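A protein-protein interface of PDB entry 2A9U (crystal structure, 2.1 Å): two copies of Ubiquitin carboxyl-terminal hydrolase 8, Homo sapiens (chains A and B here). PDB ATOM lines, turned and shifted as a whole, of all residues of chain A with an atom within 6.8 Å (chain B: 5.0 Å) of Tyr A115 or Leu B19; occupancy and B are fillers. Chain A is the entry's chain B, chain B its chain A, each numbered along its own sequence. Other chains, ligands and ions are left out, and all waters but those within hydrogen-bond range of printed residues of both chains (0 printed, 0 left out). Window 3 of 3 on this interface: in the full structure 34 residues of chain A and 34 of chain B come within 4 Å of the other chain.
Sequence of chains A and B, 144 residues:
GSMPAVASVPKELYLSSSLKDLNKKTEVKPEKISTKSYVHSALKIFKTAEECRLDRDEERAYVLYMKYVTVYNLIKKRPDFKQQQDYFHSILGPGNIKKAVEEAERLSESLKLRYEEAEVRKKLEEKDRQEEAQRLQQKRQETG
N of Ser B16 is in hydrogen-bond range of OE2 of Glu A59, at 2.9 Å. The side-chain amide oxygen (OD1) of Asn B23 sits at hydrogen-bond distance from the side-chain hydroxyl (OH) of Tyr A62 (2.5 Å).
The side-chain hydroxyl of Ser B16 lies within hydrogen-bond range of the backbone carbonyl oxygen of Ser B18, 3.1 Å away. OG of Ser B16 is in hydrogen-bond range of OD2 of Asp B21 (3.0 Å). The side-chain hydroxyl (OG) of Ser B18 lies within hydrogen-bond range of the backbone NH (N) of Asp B21 (3.1 Å). O of Leu B19 sits close to ND2 of Asn B23. OE2 of Glu A59 is in hydrogen-bond range of OH of Tyr A115, 2.5 Å away. The side-chain carboxylate (OE2) of Glu A109 is in salt-bridge range of the side-chain amino group (NZ) of Lys A112 (3.0 Å).
Glu A59 touches Leu B13. CD2 of Tyr A62 touches CD2 of Leu B22 (3.7 Å). Leu A111 touches Leu B22. Lys A112 touches Leu B19 (CE to CD2, 3.7 Å). CD1 of Tyr A115 touches CD1 of Leu B13 (3.8 Å). O of Ser B16 touches CE1 of Tyr A115, at 3.1 Å. CD1 of Tyr A115 touches C of Ser B17 (3.5 Å). CE2 of Tyr A115 touches C of Ser B18 (3.4 Å). CD2 of Tyr A115 touches N of Leu B19, at 3.4 Å. Leu B22 touches Tyr A115.
Tyr A115 touches just these residues of chain B: Leu B13 (3.8 Å), Ser B16 (3.1 Å), Ser B17 (3.5 Å), Ser B18 (3.4 Å), Leu B19 (3.4 Å) and Leu B22 (3.3 Å). Printed residues of chain A within 4 Å of Ser B16: Glu A59 and Tyr A115. Of the printed residues of chain A, Asn B23 touches Tyr A62 (2.5 Å). Of the printed residues of chain A, Leu B13 touches Glu A59 (3.6 Å), Arg A114 (3.7 Å) and Tyr A115 (3.8 Å). Of the printed residues of chain B, Tyr A62 touches Leu B22 (3.7 Å) and Asn B23 (2.5 Å). Of the printed residues of chain B, Lys A112 touches Leu B19 (3.7 Å). The nearest printed residue of chain B that does not touch Tyr A115 is Lys B20 (6.1 Å).
Hydrophobic or aromatic side chains of chain B within 4 Å of the printed part of chain A: Leu B13, Leu B19 and Leu B22. Of the 16 printed residues of chain A, 6 touch a printed residue of chain B. Hydrophobic or aromatic side chains of chain A that line the printed part of chain B: Tyr A62, Leu A111 and Tyr A115. Along chain A the printed residues that touch a printed residue of chain B span positions 59 to 115.
No position is printed for both chains. Of the 14 pairs that touch across the chains among the printed residues, none has its exchanged pair printed and touching as well.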
ATOM      1  N   GLU A  59     -22.834 -16.592   8.914  1.00  0.00           N
ATOM      2  CA  GLU A  59     -23.996 -17.283   9.509  1.00  0.00           C
ATOM      3  C   GLU A  59     -23.587 -18.460  10.397  1.00  0.00           C
ATOM      4  O   GLU A  59     -24.071 -18.561  11.525  1.00  0.00           O
ATOM      5  CB  GLU A  59     -24.948 -17.801   8.419  1.00  0.00           C
ATOM      6  CG  GLU A  59     -25.586 -16.705   7.548  1.00  0.00           C
ATOM      7  CD  GLU A  59     -26.357 -17.308   6.386  1.00  0.00           C
ATOM      8  OE1 GLU A  59     -25.691 -17.973   5.526  1.00  0.00           O
ATOM      9  OE2 GLU A  59     -27.618 -17.126   6.350  1.00  0.00           O
ATOM     10  N   TYR A  62     -21.630 -17.230  13.436  1.00  0.00           N
ATOM     11  CA  TYR A  62     -22.561 -16.614  14.390  1.00  0.00           C
ATOM     12  C   TYR A  62     -23.379 -17.676  15.177  1.00  0.00           C
ATOM     13  O   TYR A  62     -23.488 -17.601  16.406  1.00  0.00           O
ATOM     14  CB  TYR A  62     -23.525 -15.645  13.669  1.00  0.00           C
ATOM     15  CG  TYR A  62     -24.688 -15.223  14.541  1.00  0.00           C
ATOM     16  CD1 TYR A  62     -24.559 -14.151  15.447  1.00  0.00           C
ATOM     17  CD2 TYR A  62     -25.892 -15.899  14.490  1.00  0.00           C
ATOM     18  CE1 TYR A  62     -25.603 -13.773  16.263  1.00  0.00           C
ATOM     19  CE2 TYR A  62     -26.954 -15.546  15.336  1.00  0.00           C
ATOM     20  CZ  TYR A  62     -26.799 -14.479  16.210  1.00  0.00           C
ATOM     21  OH  TYR A  62     -27.839 -14.101  17.032  1.00  0.00           O
ATOM     22  N   LEU A 107     -21.057 -10.137  14.517  1.00  0.00           N
ATOM     23  CA  LEU A 107     -21.740 -10.893  13.469  1.00  0.00           C
ATOM     24  C   LEU A 107     -23.241 -10.635  13.442  1.00  0.00           C
ATOM     25  O   LEU A 107     -23.786 -10.540  12.358  1.00  0.00           O
ATOM     26  CB  LEU A 107     -21.426 -12.394  13.502  1.00  0.00           C
ATOM     27  CG  LEU A 107     -19.976 -12.830  13.287  1.00  0.00           C
ATOM     28  CD1 LEU A 107     -19.732 -14.223  13.817  1.00  0.00           C
ATOM     29  CD2 LEU A 107     -19.559 -12.748  11.828  1.00  0.00           C
ATOM     30  N   SER A 108     -23.923 -10.496  14.586  1.00  0.00           N
ATOM     31  CA  SER A 108     -25.377 -10.202  14.502  1.00  0.00           C
ATOM     32  C   SER A 108     -25.601  -8.888  13.730  1.00  0.00           C
ATOM     33  O   SER A 108     -26.444  -8.833  12.822  1.00  0.00           O
ATOM     34  CB  SER A 108     -26.070 -10.108  15.861  1.00  0.00           C
ATOM     35  OG  SER A 108     -25.679  -8.919  16.531  1.00  0.00           O
ATOM     36  N   GLU A 109     -24.822  -7.855  14.090  1.00  0.00           N
ATOM     37  CA  GLU A 109     -24.925  -6.546  13.449  1.00  0.00           C
ATOM     38  C   GLU A 109     -24.665  -6.641  11.953  1.00  0.00           C
ATOM     39  O   GLU A 109     -25.374  -6.044  11.189  1.00  0.00           O
ATOM     40  CB  GLU A 109     -24.005  -5.513  14.119  1.00  0.00           C
ATOM     41  CG  GLU A 109     -24.527  -4.964  15.477  1.00  0.00           C
ATOM     42  CD  GLU A 109     -25.887  -4.220  15.379  1.00  0.00           C
ATOM     43  OE1 GLU A 109     -25.876  -2.961  15.408  1.00  0.00           O
ATOM     44  OE2 GLU A 109     -26.955  -4.886  15.281  1.00  0.00           O
ATOM     45  N   SER A 110     -23.697  -7.455  11.546  1.00  0.00           N
ATOM     46  CA  SER A 110     -23.427  -7.697  10.123  1.00  0.00           C
ATOM     47  C   SER A 110     -24.547  -8.461   9.403  1.00  0.00           C
ATOM     48  O   SER A 110     -24.919  -8.133   8.260  1.00  0.00           O
ATOM     49  CB  SER A 110     -22.111  -8.445   9.943  1.00  0.00           C
ATOM     50  OG  SER A 110     -21.888  -8.757   8.569  1.00  0.00           O
ATOM     51  N   LEU A 111     -25.067  -9.492  10.067  1.00  0.00           N
ATOM     52  CA  LEU A 111     -26.105 -10.321   9.472  1.00  0.00           C
ATOM     53  C   LEU A 111     -27.420  -9.563   9.360  1.00  0.00           C
ATOM     54  O   LEU A 111     -28.117  -9.709   8.378  1.00  0.00           O
ATOM     55  CB  LEU A 111     -26.275 -11.641  10.264  1.00  0.00           C
ATOM     56  CG  LEU A 111     -25.080 -12.609  10.173  1.00  0.00           C
ATOM     57  CD1 LEU A 111     -25.271 -13.773  11.164  1.00  0.00           C
ATOM     58  CD2 LEU A 111     -24.929 -13.118   8.739  1.00  0.00           C
ATOM     59  N   LYS A 112     -27.764  -8.764  10.364  1.00  0.00           N
ATOM     60  CA  LYS A 112     -28.991  -7.982  10.280  1.00  0.00           C
ATOM     61  C   LYS A 112     -29.037  -7.184   8.959  1.00  0.00           C
ATOM     62  O   LYS A 112     -30.036  -7.217   8.242  1.00  0.00           O
ATOM     63  CB  LYS A 112     -29.106  -7.044  11.472  1.00  0.00           C
ATOM     64  CG  LYS A 112     -29.849  -7.640  12.654  1.00  0.00           C
ATOM     65  CD  LYS A 112     -30.087  -6.570  13.720  1.00  0.00           C
ATOM     66  CE  LYS A 112     -30.246  -7.196  15.097  1.00  0.00           C
ATOM     67  NZ  LYS A 112     -29.305  -6.587  16.073  1.00  0.00           N
ATOM     68  N   LEU A 113     -27.931  -6.514   8.634  1.00  0.00           N
ATOM     69  CA  LEU A 113     -27.838  -5.657   7.452  1.00  0.00           C
ATOM     70  C   LEU A 113     -27.808  -6.489   6.171  1.00  0.00           C
ATOM     71  O   LEU A 113     -28.412  -6.139   5.176  1.00  0.00           O
ATOM     72  CB  LEU A 113     -26.594  -4.775   7.542  1.00  0.00           C
ATOM     73  CG  LEU A 113     -26.580  -3.655   8.597  1.00  0.00           C
ATOM     74  CD1 LEU A 113     -25.149  -3.262   8.898  1.00  0.00           C
ATOM     75  CD2 LEU A 113     -27.429  -2.439   8.142  1.00  0.00           C
ATOM     76  N   ARG A 114     -27.116  -7.615   6.210  1.00  0.00           N
ATOM     77  CA  ARG A 114     -27.009  -8.441   5.039  1.00  0.00           C
ATOM     78  C   ARG A 114     -28.376  -9.074   4.712  1.00  0.00           C
ATOM     79  O   ARG A 114     -28.734  -9.196   3.528  1.00  0.00           O
ATOM     80  CB  ARG A 114     -25.896  -9.484   5.213  1.00  0.00           C
ATOM     81  CG  ARG A 114     -24.486  -8.859   5.376  1.00  0.00           C
ATOM     82  CD  ARG A 114     -23.389  -9.919   5.432  1.00  0.00           C
ATOM     83  NE  ARG A 114     -23.335 -10.791   4.247  1.00  0.00           N
ATOM     84  CZ  ARG A 114     -22.822 -12.024   4.256  1.00  0.00           C
ATOM     85  NH1 ARG A 114     -22.278 -12.491   5.376  1.00  0.00           N
ATOM     86  NH2 ARG A 114     -22.812 -12.772   3.160  1.00  0.00           N
ATOM     87  N   TYR A 115     -29.132  -9.453   5.749  1.00  0.00           N
ATOM     88  CA  TYR A 115     -30.455 -10.012   5.534  1.00  0.00           C
ATOM     89  C   TYR A 115     -31.411  -8.913   5.049  1.00  0.00           C
ATOM     90  O   TYR A 115     -32.247  -9.168   4.178  1.00  0.00           O
ATOM     91  CB  TYR A 115     -31.012 -10.671   6.798  1.00  0.00           C
ATOM     92  CG  TYR A 115     -30.351 -12.002   7.204  1.00  0.00           C
ATOM     93  CD1 TYR A 115     -30.117 -12.985   6.252  1.00  0.00           C
ATOM     94  CD2 TYR A 115     -29.991 -12.273   8.538  1.00  0.00           C
ATOM     95  CE1 TYR A 115     -29.519 -14.208   6.577  1.00  0.00           C
ATOM     96  CE2 TYR A 115     -29.399 -13.520   8.896  1.00  0.00           C
ATOM     97  CZ  TYR A 115     -29.174 -14.474   7.884  1.00  0.00           C
ATOM     98  OH  TYR A 115     -28.590 -15.693   8.125  1.00  0.00           O
ATOM     99  N   GLU A 116     -31.305  -7.719   5.638  1.00  0.00           N
ATOM    100  CA  GLU A 116     -32.156  -6.582   5.242  1.00  0.00           C
ATOM    101  C   GLU A 116     -31.881  -6.192   3.783  1.00  0.00           C
ATOM    102  O   GLU A 116     -32.803  -6.099   3.003  1.00  0.00           O
ATOM    103  CB  GLU A 116     -32.030  -5.383   6.195  1.00  0.00           C
ATOM    104  CG  GLU A 116     -33.078  -4.266   5.949  1.00  0.00           C
ATOM    105  CD  GLU A 116     -32.835  -3.003   6.770  1.00  0.00           C
ATOM    106  OE1 GLU A 116     -31.885  -2.990   7.585  1.00  0.00           O
ATOM    107  OE2 GLU A 116     -33.572  -1.995   6.605  1.00  0.00           O
ATOM    108  N   GLU A 117     -30.616  -6.005   3.429  1.00  0.00           N
ATOM    109  CA  GLU A 117     -30.197  -5.806   2.043  1.00  0.00           C
ATOM    110  C   GLU A 117     -30.815  -6.820   1.081  1.00  0.00           C
ATOM    111  O   GLU A 117     -31.541  -6.434   0.147  1.00  0.00           O
ATOM    112  CB  GLU A 117     -28.674  -5.878   1.934  1.00  0.00           C
ATOM    113  CG  GLU A 117     -28.072  -5.196   0.690  1.00  0.00           C
ATOM    114  CD  GLU A 117     -28.235  -5.985  -0.619  1.00  0.00           C
ATOM    115  OE1 GLU A 117     -27.877  -7.198  -0.657  1.00  0.00           O
ATOM    116  OE2 GLU A 117     -28.705  -5.376  -1.624  1.00  0.00           O
ATOM    117  N   ALA A 118     -30.518  -8.106   1.284  1.00  0.00           N
ATOM    118  CA  ALA A 118     -31.037  -9.149   0.385  1.00  0.00           C
ATOM    119  C   ALA A 118     -32.563  -9.073   0.218  1.00  0.00           C
ATOM    120  O   ALA A 118     -33.061  -9.231  -0.890  1.00  0.00           O
ATOM    121  CB  ALA A 118     -30.602 -10.548   0.826  1.00  0.00           C
ATOM    122  N   GLU A 119     -33.289  -8.843   1.308  1.00  0.00           N
ATOM    123  CA  GLU A 119     -34.748  -8.649   1.259  1.00  0.00           C
ATOM    124  C   GLU A 119     -35.188  -7.379   0.463  1.00  0.00           C
ATOM    125  O   GLU A 119     -36.048  -7.468  -0.410  1.00  0.00           O
ATOM    126  CB  GLU A 119     -35.313  -8.650   2.683  1.00  0.00           C
ATOM    127  CG  GLU A 119     -36.857  -8.714   2.797  1.00  0.00           C
ATOM    128  CD  GLU A 119     -37.487 -10.056   2.333  1.00  0.00           C
ATOM    129  OE1 GLU A 119     -36.817 -11.121   2.430  1.00  0.00           O
ATOM    130  OE2 GLU A 119     -38.664 -10.035   1.879  1.00  0.00           O
ATOM    131  N   VAL A 120     -34.593  -6.212   0.741  1.00  0.00           N
ATOM    132  CA  VAL A 120     -34.886  -5.011  -0.063  1.00  0.00           C
ATOM    133  C   VAL A 120     -34.580  -5.241  -1.564  1.00  0.00           C
ATOM    134  O   VAL A 120     -35.431  -4.980  -2.444  1.00  0.00           O
ATOM    135  CB  VAL A 120     -34.142  -3.750   0.446  1.00  0.00           C
ATOM    136  CG1 VAL A 120     -34.642  -2.512  -0.310  1.00  0.00           C
ATOM    137  CG2 VAL A 120     -34.413  -3.549   1.909  1.00  0.00           C
ATOM    138  N   LEU B  13     -24.748 -15.647   1.510  1.00  0.00           N
ATOM    139  CA  LEU B  13     -25.754 -16.112   2.459  1.00  0.00           C
ATOM    140  C   LEU B  13     -26.377 -17.390   1.928  1.00  0.00           C
ATOM    141  O   LEU B  13     -26.622 -17.500   0.732  1.00  0.00           O
ATOM    142  CB  LEU B  13     -26.826 -15.042   2.663  1.00  0.00           C
ATOM    143  CG  LEU B  13     -26.396 -13.769   3.425  1.00  0.00           C
ATOM    144  CD1 LEU B  13     -27.552 -12.793   3.518  1.00  0.00           C
ATOM    145  CD2 LEU B  13     -25.859 -14.083   4.838  1.00  0.00           C
ATOM    146  N   SER B  16     -29.758 -19.110   6.142  1.00  0.00           N
ATOM    147  CA  SER B  16     -31.023 -18.562   6.552  1.00  0.00           C
ATOM    148  C   SER B  16     -31.343 -17.259   5.804  1.00  0.00           C
ATOM    149  O   SER B  16     -30.504 -16.719   5.033  1.00  0.00           O
ATOM    150  CB  SER B  16     -31.019 -18.379   8.068  1.00  0.00           C
ATOM    151  OG  SER B  16     -32.297 -18.007   8.532  1.00  0.00           O
ATOM    152  N   SER B  17     -32.554 -16.746   6.019  1.00  0.00           N
ATOM    153  CA  SER B  17     -32.919 -15.456   5.441  1.00  0.00           C
ATOM    154  C   SER B  17     -33.275 -14.423   6.488  1.00  0.00           C
ATOM    155  O   SER B  17     -33.664 -13.311   6.148  1.00  0.00           O
ATOM    156  CB  SER B  17     -34.056 -15.616   4.441  1.00  0.00           C
ATOM    157  OG  SER B  17     -35.249 -15.906   5.134  1.00  0.00           O
ATOM    158  N   SER B  18     -33.113 -14.769   7.766  1.00  0.00           N
ATOM    159  CA  SER B  18     -33.298 -13.792   8.844  1.00  0.00           C
ATOM    160  C   SER B  18     -32.504 -14.177  10.048  1.00  0.00           C
ATOM    161  O   SER B  18     -32.155 -15.358  10.221  1.00  0.00           O
ATOM    162  CB  SER B  18     -34.786 -13.663   9.245  1.00  0.00           C
ATOM    163  OG  SER B  18     -35.261 -14.893   9.760  1.00  0.00           O
ATOM    164  N   LEU B  19     -32.247 -13.192  10.905  1.00  0.00           N
ATOM    165  CA  LEU B  19     -31.618 -13.453  12.194  1.00  0.00           C
ATOM    166  C   LEU B  19     -32.505 -14.283  13.117  1.00  0.00           C
ATOM    167  O   LEU B  19     -32.004 -15.109  13.898  1.00  0.00           O
ATOM    168  CB  LEU B  19     -31.223 -12.154  12.890  1.00  0.00           C
ATOM    169  CG  LEU B  19     -30.066 -12.239  13.884  1.00  0.00           C
ATOM    170  CD1 LEU B  19     -28.750 -12.649  13.224  1.00  0.00           C
ATOM    171  CD2 LEU B  19     -29.928 -10.869  14.539  1.00  0.00           C
ATOM    172  N   LYS B  20     -33.812 -14.059  13.016  1.00  0.00           N
ATOM    173  CA  LYS B  20     -34.807 -14.771  13.810  1.00  0.00           C
ATOM    174  C   LYS B  20     -34.772 -16.264  13.504  1.00  0.00           C
ATOM    175  O   LYS B  20     -34.822 -17.088  14.432  1.00  0.00           O
ATOM    176  CB  LYS B  20     -36.221 -14.223  13.545  1.00  0.00           C
ATOM    177  CG  LYS B  20     -37.152 -14.380  14.737  1.00  0.00           C
ATOM    178  CD  LYS B  20     -38.595 -13.905  14.470  1.00  0.00           C
ATOM    179  CE  LYS B  20     -39.525 -15.103  14.282  1.00  0.00           C
ATOM    180  NZ  LYS B  20     -40.907 -14.790  14.813  1.00  0.00           N
ATOM    181  N   ASP B  21     -34.701 -16.614  12.221  1.00  0.00           N
ATOM    182  CA  ASP B  21     -34.651 -18.026  11.815  1.00  0.00           C
ATOM    183  C   ASP B  21     -33.308 -18.598  12.221  1.00  0.00           C
ATOM    184  O   ASP B  21     -33.247 -19.676  12.793  1.00  0.00           O
ATOM    185  CB  ASP B  21     -34.864 -18.217  10.308  1.00  0.00           C
ATOM    186  CG  ASP B  21     -34.905 -19.719   9.894  1.00  0.00           C
ATOM    187  OD1 ASP B  21     -36.020 -20.306   9.941  1.00  0.00           O
ATOM    188  OD2 ASP B  21     -33.845 -20.321   9.526  1.00  0.00           O
ATOM    189  N   LEU B  22     -32.234 -17.856  11.937  1.00  0.00           N
ATOM    190  CA  LEU B  22     -30.868 -18.260  12.289  1.00  0.00           C
ATOM    191  C   LEU B  22     -30.728 -18.481  13.786  1.00  0.00           C
ATOM    192  O   LEU B  22     -30.099 -19.441  14.194  1.00  0.00           O
ATOM    193  CB  LEU B  22     -29.871 -17.195  11.810  1.00  0.00           C
ATOM    194  CG  LEU B  22     -28.428 -17.625  11.605  1.00  0.00           C
ATOM    195  CD1 LEU B  22     -28.288 -18.782  10.581  1.00  0.00           C
ATOM    196  CD2 LEU B  22     -27.596 -16.377  11.215  1.00  0.00           C
ATOM    197  N   ASN B  23     -31.372 -17.638  14.606  1.00  0.00           N
ATOM    198  CA  ASN B  23     -31.328 -17.819  16.057  1.00  0.00           C
ATOM    199  C   ASN B  23     -31.881 -19.145  16.572  1.00  0.00           C
ATOM    200  O   ASN B  23     -31.498 -19.597  17.662  1.00  0.00           O
ATOM    201  CB  ASN B  23     -31.987 -16.664  16.795  1.00  0.00           C
ATOM    202  CG  ASN B  23     -31.105 -15.447  16.870  1.00  0.00           C
ATOM    203  OD1 ASN B  23     -29.889 -15.545  16.834  1.00  0.00           O
ATOM    204  ND2 ASN B  23     -31.716 -14.281  16.983  1.00  0.00           N
